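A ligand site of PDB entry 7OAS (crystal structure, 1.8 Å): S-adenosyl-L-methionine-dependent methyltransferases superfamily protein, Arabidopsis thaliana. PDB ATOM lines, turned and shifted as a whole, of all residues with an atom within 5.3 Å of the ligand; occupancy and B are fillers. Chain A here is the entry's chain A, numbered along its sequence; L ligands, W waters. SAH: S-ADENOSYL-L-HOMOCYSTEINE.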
ATOM      1  N   LEU A  28      27.937 -12.014   3.009  1.00  0.00           N
ATOM      2  CA  LEU A  28      27.155 -11.882   1.786  1.00  0.00           C
ATOM      3  C   LEU A  28      26.571 -13.216   1.344  1.00  0.00           C
ATOM      4  O   LEU A  28      25.422 -13.292   0.901  1.00  0.00           O
ATOM      5  CB  LEU A  28      28.014 -11.288   0.675  1.00  0.00           C
ATOM      6  CG  LEU A  28      28.432  -9.814   0.863  1.00  0.00           C
ATOM      7  CD1 LEU A  28      29.285  -9.360  -0.305  1.00  0.00           C
ATOM      8  CD2 LEU A  28      27.215  -8.922   1.022  1.00  0.00           C
ATOM      9  N   GLY A  29      27.344 -14.298   1.471  1.00  0.00           N
ATOM     10  CA  GLY A  29      26.918 -15.604   1.002  1.00  0.00           C
ATOM     11  C   GLY A  29      25.808 -16.251   1.804  1.00  0.00           C
ATOM     12  O   GLY A  29      25.308 -17.306   1.375  1.00  0.00           O
ATOM     13  N   THR A  31      22.842 -15.205   2.098  1.00  0.00           N
ATOM     14  CA  THR A  31      21.579 -14.817   1.488  1.00  0.00           C
ATOM     15  C   THR A  31      21.566 -15.284   0.041  1.00  0.00           C
ATOM     16  O   THR A  31      22.611 -15.269  -0.622  1.00  0.00           O
ATOM     17  CB  THR A  31      21.383 -13.282   1.584  1.00  0.00           C
ATOM     18  OG1 THR A  31      21.156 -12.913   2.944  1.00  0.00           O
ATOM     19  CG2 THR A  31      20.211 -12.814   0.728  1.00  0.00           C
ATOM     20  N   VAL A  32      20.412 -15.738  -0.441  1.00  0.00           N
ATOM     21  CA  VAL A  32      20.284 -16.119  -1.842  1.00  0.00           C
ATOM     22  C   VAL A  32      20.177 -14.865  -2.697  1.00  0.00           C
ATOM     23  O   VAL A  32      19.310 -14.011  -2.467  1.00  0.00           O
ATOM     24  CB  VAL A  32      19.061 -17.035  -2.039  1.00  0.00           C
ATOM     25  CG1 VAL A  32      18.812 -17.234  -3.536  1.00  0.00           C
ATOM     26  CG2 VAL A  32      19.274 -18.386  -1.336  1.00  0.00           C
ATOM     27  N   TRP A  33      21.052 -14.748  -3.693  1.00  0.00           N
ATOM     28  CA  TRP A  33      21.079 -13.605  -4.593  1.00  0.00           C
ATOM     29  C   TRP A  33      20.372 -13.917  -5.914  1.00  0.00           C
ATOM     30  O   TRP A  33      20.352 -15.064  -6.367  1.00  0.00           O
ATOM     31  CB  TRP A  33      22.520 -13.155  -4.847  1.00  0.00           C
ATOM     32  CG  TRP A  33      23.130 -12.604  -3.576  1.00  0.00           C
ATOM     33  CD1 TRP A  33      23.794 -13.313  -2.624  1.00  0.00           C
ATOM     34  CD2 TRP A  33      23.082 -11.251  -3.111  1.00  0.00           C
ATOM     35  NE1 TRP A  33      24.182 -12.491  -1.596  1.00  0.00           N
ATOM     36  CE2 TRP A  33      23.764 -11.216  -1.871  1.00  0.00           C
ATOM     37  CE3 TRP A  33      22.558 -10.060  -3.621  1.00  0.00           C
ATOM     38  CZ2 TRP A  33      23.908 -10.043  -1.135  1.00  0.00           C
ATOM     39  CZ3 TRP A  33      22.700  -8.896  -2.887  1.00  0.00           C
ATOM     40  CH2 TRP A  33      23.378  -8.890  -1.656  1.00  0.00           C
ATOM     41  N   ALA A  35      20.872 -13.538  -9.025  1.00  0.00           N
ATOM     42  CA  ALA A  35      21.566 -14.145 -10.157  1.00  0.00           C
ATOM     43  C   ALA A  35      21.577 -15.663 -10.079  1.00  0.00           C
ATOM     44  O   ALA A  35      21.533 -16.343 -11.107  1.00  0.00           O
ATOM     45  CB  ALA A  35      22.997 -13.637 -10.245  1.00  0.00           C
ATOM     46  N   SER A  36      21.677 -16.231  -8.871  1.00  0.00           N
ATOM     47  CA  SER A  36      21.668 -17.688  -8.774  1.00  0.00           C
ATOM     48  C   SER A  36      20.318 -18.250  -9.222  1.00  0.00           C
ATOM     49  O   SER A  36      20.260 -19.306  -9.860  1.00  0.00           O
ATOM     50  CB  SER A  36      22.023 -18.160  -7.371  1.00  0.00           C
ATOM     51  OG  SER A  36      21.011 -17.827  -6.442  1.00  0.00           O
ATOM     52  N   GLU A  64      31.512 -24.914  -8.684  1.00  0.00           N
ATOM     53  CA  GLU A  64      30.884 -23.629  -8.424  1.00  0.00           C
ATOM     54  C   GLU A  64      31.771 -22.824  -7.472  1.00  0.00           C
ATOM     55  O   GLU A  64      32.203 -23.328  -6.428  1.00  0.00           O
ATOM     56  CB  GLU A  64      29.490 -23.776  -7.831  1.00  0.00           C
ATOM     57  CG  GLU A  64      28.913 -22.376  -7.449  1.00  0.00           C
ATOM     58  CD  GLU A  64      27.416 -22.357  -7.157  1.00  0.00           C
ATOM     59  OE1 GLU A  64      26.843 -23.434  -6.902  1.00  0.00           O
ATOM     60  OE2 GLU A  64      26.824 -21.257  -7.182  1.00  0.00           O
ATOM     61  N   LEU A  65      32.041 -21.586  -7.844  1.00  0.00           N
ATOM     62  CA  LEU A  65      32.804 -20.682  -6.990  1.00  0.00           C
ATOM     63  C   LEU A  65      31.857 -19.703  -6.322  1.00  0.00           C
ATOM     64  O   LEU A  65      30.911 -19.217  -6.952  1.00  0.00           O
ATOM     65  CB  LEU A  65      33.833 -19.920  -7.822  1.00  0.00           C
ATOM     66  CG  LEU A  65      34.798 -20.807  -8.597  1.00  0.00           C
ATOM     67  CD1 LEU A  65      35.693 -19.938  -9.479  1.00  0.00           C
ATOM     68  CD2 LEU A  65      35.646 -21.613  -7.615  1.00  0.00           C
ATOM     69  N   GLY A  66      32.106 -19.433  -5.032  1.00  0.00           N
ATOM     70  CA  GLY A  66      31.296 -18.513  -4.231  1.00  0.00           C
ATOM     71  C   GLY A  66      29.848 -18.957  -4.175  1.00  0.00           C
ATOM     72  O   GLY A  66      28.928 -18.151  -4.401  1.00  0.00           O
ATOM     73  N   ALA A  67      29.609 -20.246  -3.894  1.00  0.00           N
ATOM     74  CA  ALA A  67      28.265 -20.796  -3.991  1.00  0.00           C
ATOM     75  C   ALA A  67      27.275 -20.188  -3.010  1.00  0.00           C
ATOM     76  O   ALA A  67      26.071 -20.234  -3.280  1.00  0.00           O
ATOM     77  CB  ALA A  67      28.301 -22.301  -3.792  1.00  0.00           C
ATOM     78  N   GLY A  68      27.743 -19.661  -1.874  1.00  0.00           N
ATOM     79  CA  GLY A  68      26.832 -19.122  -0.873  1.00  0.00           C
ATOM     80  C   GLY A  68      25.898 -20.212  -0.365  1.00  0.00           C
ATOM     81  O   GLY A  68      26.321 -21.275   0.114  1.00  0.00           O
ATOM     82  N   CYS A  69      24.585 -19.952  -0.480  1.00  0.00           N
ATOM     83  CA  CYS A  69      23.570 -20.896  -0.036  1.00  0.00           C
ATOM     84  C   CYS A  69      23.444 -22.099  -0.966  1.00  0.00           C
ATOM     85  O   CYS A  69      22.904 -23.127  -0.536  1.00  0.00           O
ATOM     86  CB  CYS A  69      22.225 -20.177   0.127  1.00  0.00           C
ATOM     87  SG  CYS A  69      22.207 -18.843   1.398  1.00  0.00           S
ATOM     88  N   ASP A  87      32.996 -22.416  -1.239  1.00  0.00           N
ATOM     89  CA  ASP A  87      32.962 -21.071  -0.681  1.00  0.00           C
ATOM     90  C   ASP A  87      34.015 -21.004   0.414  1.00  0.00           C
ATOM     91  O   ASP A  87      34.795 -21.946   0.597  1.00  0.00           O
ATOM     92  CB  ASP A  87      31.556 -20.729  -0.170  1.00  0.00           C
ATOM     93  CG  ASP A  87      31.235 -19.255  -0.308  1.00  0.00           C
ATOM     94  OD1 ASP A  87      31.944 -18.438   0.330  1.00  0.00           O
ATOM     95  OD2 ASP A  87      30.285 -18.915  -1.048  1.00  0.00           O
ATOM     96  N   GLN A  88      34.045 -19.883   1.131  1.00  0.00           N
ATOM     97  CA  GLN A  88      34.962 -19.775   2.258  1.00  0.00           C
ATOM     98  C   GLN A  88      34.380 -20.500   3.467  1.00  0.00           C
ATOM     99  O   GLN A  88      33.183 -20.776   3.549  1.00  0.00           O
ATOM    100  CB  GLN A  88      35.211 -18.309   2.590  1.00  0.00           C
ATOM    101  CG  GLN A  88      35.381 -17.438   1.367  1.00  0.00           C
ATOM    102  CD  GLN A  88      35.806 -16.020   1.744  1.00  0.00           C
ATOM    103  OE1 GLN A  88      36.995 -15.747   1.928  1.00  0.00           O
ATOM    104  NE2 GLN A  88      34.839 -15.113   1.876  1.00  0.00           N
ATOM    105  N   VAL A  91      31.017 -19.743   5.226  1.00  0.00           N
ATOM    106  CA  VAL A  91      29.792 -20.059   4.522  1.00  0.00           C
ATOM    107  C   VAL A  91      29.521 -21.563   4.438  1.00  0.00           C
ATOM    108  O   VAL A  91      28.366 -21.966   4.252  1.00  0.00           O
ATOM    109  CB  VAL A  91      29.850 -19.413   3.118  1.00  0.00           C
ATOM    110  CG1 VAL A  91      28.779 -19.964   2.175  1.00  0.00           C
ATOM    111  CG2 VAL A  91      29.739 -17.901   3.249  1.00  0.00           C
ATOM    112  N   LEU A 123      37.154 -23.367  -0.746  1.00  0.00           N
ATOM    113  CA  LEU A 123      38.019 -22.824  -1.791  1.00  0.00           C
ATOM    114  C   LEU A 123      38.060 -21.303  -1.656  1.00  0.00           C
ATOM    115  O   LEU A 123      37.178 -20.598  -2.165  1.00  0.00           O
ATOM    116  CB  LEU A 123      37.566 -23.246  -3.185  1.00  0.00           C
ATOM    117  CG  LEU A 123      38.642 -23.246  -4.275  1.00  0.00           C
ATOM    118  CD1 LEU A 123      38.178 -24.043  -5.492  1.00  0.00           C
ATOM    119  CD2 LEU A 123      39.045 -21.812  -4.697  1.00  0.00           C
ATOM    120  N   ASP A 124      39.118 -20.804  -0.994  1.00  0.00           N
ATOM    121  CA  ASP A 124      39.457 -19.385  -1.012  1.00  0.00           C
ATOM    122  C   ASP A 124      40.087 -19.016  -2.358  1.00  0.00           C
ATOM    123  O   ASP A 124      41.109 -19.604  -2.744  1.00  0.00           O
ATOM    124  CB  ASP A 124      40.430 -19.051   0.107  1.00  0.00           C
ATOM    125  CG  ASP A 124      39.828 -19.199   1.474  1.00  0.00           C
ATOM    126  OD1 ASP A 124      38.601 -19.082   1.593  1.00  0.00           O
ATOM    127  OD2 ASP A 124      40.585 -19.440   2.436  1.00  0.00           O
ATOM    128  N   TRP A 125      39.531 -18.029  -3.054  1.00  0.00           N
ATOM    129  CA  TRP A 125      40.016 -17.736  -4.396  1.00  0.00           C
ATOM    130  C   TRP A 125      41.495 -17.401  -4.345  1.00  0.00           C
ATOM    131  O   TRP A 125      41.948 -16.661  -3.463  1.00  0.00           O
ATOM    132  CB  TRP A 125      39.219 -16.597  -5.029  1.00  0.00           C
ATOM    133  CG  TRP A 125      37.743 -16.933  -5.146  1.00  0.00           C
ATOM    134  CD1 TRP A 125      37.177 -18.184  -5.092  1.00  0.00           C
ATOM    135  CD2 TRP A 125      36.674 -16.011  -5.339  1.00  0.00           C
ATOM    136  NE1 TRP A 125      35.814 -18.086  -5.238  1.00  0.00           N
ATOM    137  CE2 TRP A 125      35.483 -16.756  -5.382  1.00  0.00           C
ATOM    138  CE3 TRP A 125      36.604 -14.612  -5.450  1.00  0.00           C
ATOM    139  CZ2 TRP A 125      34.235 -16.150  -5.559  1.00  0.00           C
ATOM    140  CZ3 TRP A 125      35.362 -14.018  -5.623  1.00  0.00           C
ATOM    141  CH2 TRP A 125      34.199 -14.771  -5.655  1.00  0.00           C
ATOM    142  N   THR A 144      27.716 -17.282  -9.618  1.00  0.00           N
ATOM    143  CA  THR A 144      26.611 -16.342  -9.745  1.00  0.00           C
ATOM    144  C   THR A 144      26.762 -15.250  -8.701  1.00  0.00           C
ATOM    145  O   THR A 144      26.937 -15.538  -7.516  1.00  0.00           O
ATOM    146  CB  THR A 144      25.238 -17.034  -9.633  1.00  0.00           C
ATOM    147  OG1 THR A 144      25.114 -17.674  -8.357  1.00  0.00           O
ATOM    148  CG2 THR A 144      25.060 -18.084 -10.737  1.00  0.00           C
ATOM    149  N   ASP A 145      26.654 -14.007  -9.160  1.00  0.00           N
ATOM    150  CA  ASP A 145      26.857 -12.797  -8.363  1.00  0.00           C
ATOM    151  C   ASP A 145      28.128 -12.893  -7.533  1.00  0.00           C
ATOM    152  O   ASP A 145      28.158 -12.607  -6.334  1.00  0.00           O
ATOM    153  CB  ASP A 145      25.645 -12.498  -7.474  1.00  0.00           C
ATOM    154  CG  ASP A 145      25.447 -11.019  -7.224  1.00  0.00           C
ATOM    155  OD1 ASP A 145      26.103 -10.221  -7.927  1.00  0.00           O
ATOM    156  OD2 ASP A 145      24.599 -10.686  -6.375  1.00  0.00           O
ATOM    157  N   VAL A 146      29.220 -13.260  -8.202  1.00  0.00           N
ATOM    158  CA  VAL A 146      30.539 -13.299  -7.592  1.00  0.00           C
ATOM    159  C   VAL A 146      31.421 -12.145  -8.043  1.00  0.00           C
ATOM    160  O   VAL A 146      32.572 -12.045  -7.607  1.00  0.00           O
ATOM    161  CB  VAL A 146      31.223 -14.640  -7.864  1.00  0.00           C
ATOM    162  CG1 VAL A 146      30.523 -15.741  -7.073  1.00  0.00           C
ATOM    163  CG2 VAL A 146      31.197 -14.961  -9.340  1.00  0.00           C
ATOM    164  N   TYR A 148      31.530  -8.106  -7.845  1.00  0.00           N
ATOM    165  CA  TYR A 148      30.930  -6.925  -7.247  1.00  0.00           C
ATOM    166  C   TYR A 148      31.964  -5.942  -6.720  1.00  0.00           C
ATOM    167  O   TYR A 148      31.679  -4.746  -6.611  1.00  0.00           O
ATOM    168  CB  TYR A 148      29.970  -7.302  -6.111  1.00  0.00           C
ATOM    169  CG  TYR A 148      30.502  -8.311  -5.112  1.00  0.00           C
ATOM    170  CD1 TYR A 148      30.323  -9.685  -5.323  1.00  0.00           C
ATOM    171  CD2 TYR A 148      31.101  -7.911  -3.930  1.00  0.00           C
ATOM    172  CE1 TYR A 148      30.781 -10.608  -4.405  1.00  0.00           C
ATOM    173  CE2 TYR A 148      31.546  -8.836  -2.997  1.00  0.00           C
ATOM    174  CZ  TYR A 148      31.389 -10.180  -3.252  1.00  0.00           C
ATOM    175  OH  TYR A 148      31.839 -11.109  -2.344  1.00  0.00           O
ATOM    176  N   LEU A 152      38.228  -8.121  -5.989  1.00  0.00           N
ATOM    177  CA  LEU A 152      37.998  -9.550  -6.133  1.00  0.00           C
ATOM    178  C   LEU A 152      38.033 -10.021  -7.590  1.00  0.00           C
ATOM    179  O   LEU A 152      37.872 -11.219  -7.838  1.00  0.00           O
ATOM    180  CB  LEU A 152      36.653  -9.954  -5.508  1.00  0.00           C
ATOM    181  CG  LEU A 152      36.505  -9.810  -3.990  1.00  0.00           C
ATOM    182  CD1 LEU A 152      35.092 -10.147  -3.526  1.00  0.00           C
ATOM    183  CD2 LEU A 152      37.522 -10.667  -3.244  1.00  0.00           C
HETATM  184  N   SAH L   1      26.549 -17.565  -5.544  1.00  0.00           N
HETATM  185  CA  SAH L   1      25.636 -17.221  -4.453  1.00  0.00           C
HETATM  186  CB  SAH L   1      26.317 -16.251  -3.459  1.00  0.00           C
HETATM  187  CG  SAH L   1      26.943 -14.996  -4.061  1.00  0.00           C
HETATM  188  SD  SAH L   1      27.388 -13.793  -2.781  1.00  0.00           S
HETATM  189  C   SAH L   1      24.364 -16.590  -4.991  1.00  0.00           C
HETATM  190  O   SAH L   1      24.311 -16.235  -6.175  1.00  0.00           O
HETATM  191  OXT SAH L   1      23.390 -16.415  -4.259  1.00  0.00           O
HETATM  192  C5' SAH L   1      29.173 -13.899  -3.096  1.00  0.00           C
HETATM  193  C4' SAH L   1      29.790 -15.200  -2.615  1.00  0.00           C
HETATM  194  O4' SAH L   1      31.154 -15.191  -3.012  1.00  0.00           O
HETATM  195  C3' SAH L   1      29.767 -15.318  -1.091  1.00  0.00           C
HETATM  196  O3' SAH L   1      29.289 -16.589  -0.684  1.00  0.00           O
HETATM  197  C2' SAH L   1      31.221 -15.165  -0.695  1.00  0.00           C
HETATM  198  O2' SAH L   1      31.552 -15.957   0.414  1.00  0.00           O
HETATM  199  C1' SAH L   1      31.944 -15.637  -1.943  1.00  0.00           C
HETATM  200  N9  SAH L   1      33.290 -15.049  -1.974  1.00  0.00           N
HETATM  201  C8  SAH L   1      33.634 -13.728  -1.947  1.00  0.00           C
HETATM  202  N7  SAH L   1      34.987 -13.632  -1.956  1.00  0.00           N
HETATM  203  C5  SAH L   1      35.494 -14.888  -1.967  1.00  0.00           C
HETATM  204  C6  SAH L   1      36.790 -15.394  -1.976  1.00  0.00           C
HETATM  205  N6  SAH L   1      37.839 -14.566  -1.969  1.00  0.00           N
HETATM  206  N1  SAH L   1      36.985 -16.756  -1.977  1.00  0.00           N
HETATM  207  C2  SAH L   1      35.912 -17.617  -1.971  1.00  0.00           C
HETATM  208  N3  SAH L   1      34.630 -17.113  -1.963  1.00  0.00           N
HETATM  209  C4  SAH L   1      34.438 -15.782  -1.964  1.00  0.00           C
HETATM  210  O   HOH W   1      22.418 -19.539  -3.788  1.00  0.00           O
HETATM  211  O   HOH W   2      23.415 -17.566  -1.886  1.00  0.00           O
HETATM  212  O   HOH W   3      39.089 -12.207  -0.249  1.00  0.00           O
HETATM  213  O   HOH W   4      30.001 -14.498   2.387  1.00  0.00           O
HETATM  214  O   HOH W   5      24.591 -20.200  -6.056  1.00  0.00           O
HETATM  215  O   HOH W   6      40.484 -15.065  -1.607  1.00  0.00           O
HETATM  216  O   HOH W   7      35.692 -11.843  -0.039  1.00  0.00           O
HETATM  217  O   HOH W   8      28.296 -18.884  -7.409  1.00  0.00           O
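O of Asp 87 lies within hydrogen-bond range of N of Leu 123. OD2 of Asp 87 lies within hydrogen-bond range of N of Ala 67, 3.2 Å away. N of Gly 68 sits at hydrogen-bond distance from OD2 of Asp 87 (2.8 Å). OG of Ser 36 lies within hydrogen-bond range of O of Trp 33 (2.8 Å). The indole nitrogen of Trp 33 lies close to the backbone carbonyl oxygen of Thr 31 (3.3 Å). The backbone carbonyl oxygen (O) of Leu 28 lies within hydrogen-bond range of the indole nitrogen (NE1) of Trp 33. The backbone carbonyl oxygen (O) of Gly 29 lies within hydrogen-bond range of the backbone NH (N) of Cys 69. N of Thr 31 lies within hydrogen-bond range of SG of Cys 69 (3.8 Å).
Water W2 lies within hydrogen-bond range of OXT of the ligand, O of Thr 31 and N of Cys 69. Water W6 bridges a nitrogen (N6) of the ligand and the backbone carbonyl oxygen (O) of Trp 125. Water W4 lies within hydrogen-bond range of N of Gly 29 (2.8 Å), O2' of the ligand (2.9 Å) and N of Leu 28 (3.3 Å). Water W1 lies within hydrogen-bond range of OXT of the ligand (3.3 Å) and OG of Ser 36 (3.5 Å). Water W5 lies within hydrogen-bond range of OE2 of Glu 64 (2.7 Å), O of Ala 67 (3.1 Å), N of the ligand (3.3 Å) and OG1 of Thr 144 (3.5 Å).
An oxygen (O2') of the ligand is in hydrogen-bond range of the side-chain carboxylate (OD1) of Asp 87 (2.5 Å). The backbone carbonyl oxygen (O) of Gly 66 lies within hydrogen-bond range of a nitrogen (N) of the ligand. O of Thr 144 sits at hydrogen-bond distance from N of the ligand (2.9 Å). An oxygen (O) of the ligand lies within hydrogen-bond range of the side-chain hydroxyl of Thr 144 (2.7 Å). An oxygen (OXT) of the ligand sits at hydrogen-bond distance from the backbone NH (N) of Trp 33, at 2.9 Å. NE1 of Trp 33 lies close to SD of the ligand, at 3.7 Å. The backbone NH (N) of Trp 125 lies within hydrogen-bond range of a nitrogen (N1) of the ligand, 3.0 Å away.
CA of Gly 29 touches O3' of the ligand (3.1 Å). Thr 31 touches the ligand (O to OXT, 3.9 Å). C of Val 32 touches OXT of the ligand, at 3.9 Å. CB of Ser 36 touches O of the ligand (3.2 Å). O of Ala 67 touches CA of the ligand (3.3 Å). Gly 68 touches the ligand (CA to O3', 3.5 Å). Gln 88 touches the ligand. Val 91 touches the ligand (CG2 to O2', 3.9 Å). Leu 123 touches the ligand (O to C2, 3.2 Å). CA of Asp 124 touches N1 of the ligand (3.7 Å). O of Asp 145 touches CG of the ligand, at 3.5 Å. OH of Tyr 148 touches C8 of the ligand (3.2 Å). Leu 152 touches the ligand. Hydrophobic or aromatic side chains that line the ligand: Trp 33, Val 91, Trp 125, Tyr 148 and Leu 152. 18 residues have an atom within 4 Å of the ligand: Gly 29, Thr 31, Val 32, Trp 33, Ser 36, Gly 66, Ala 67, Gly 68, Asp 87, Gln 88, Val 91, Leu 123, Asp 124, Trp 125, Thr 144, Asp 145, Tyr 148 and Leu 152.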
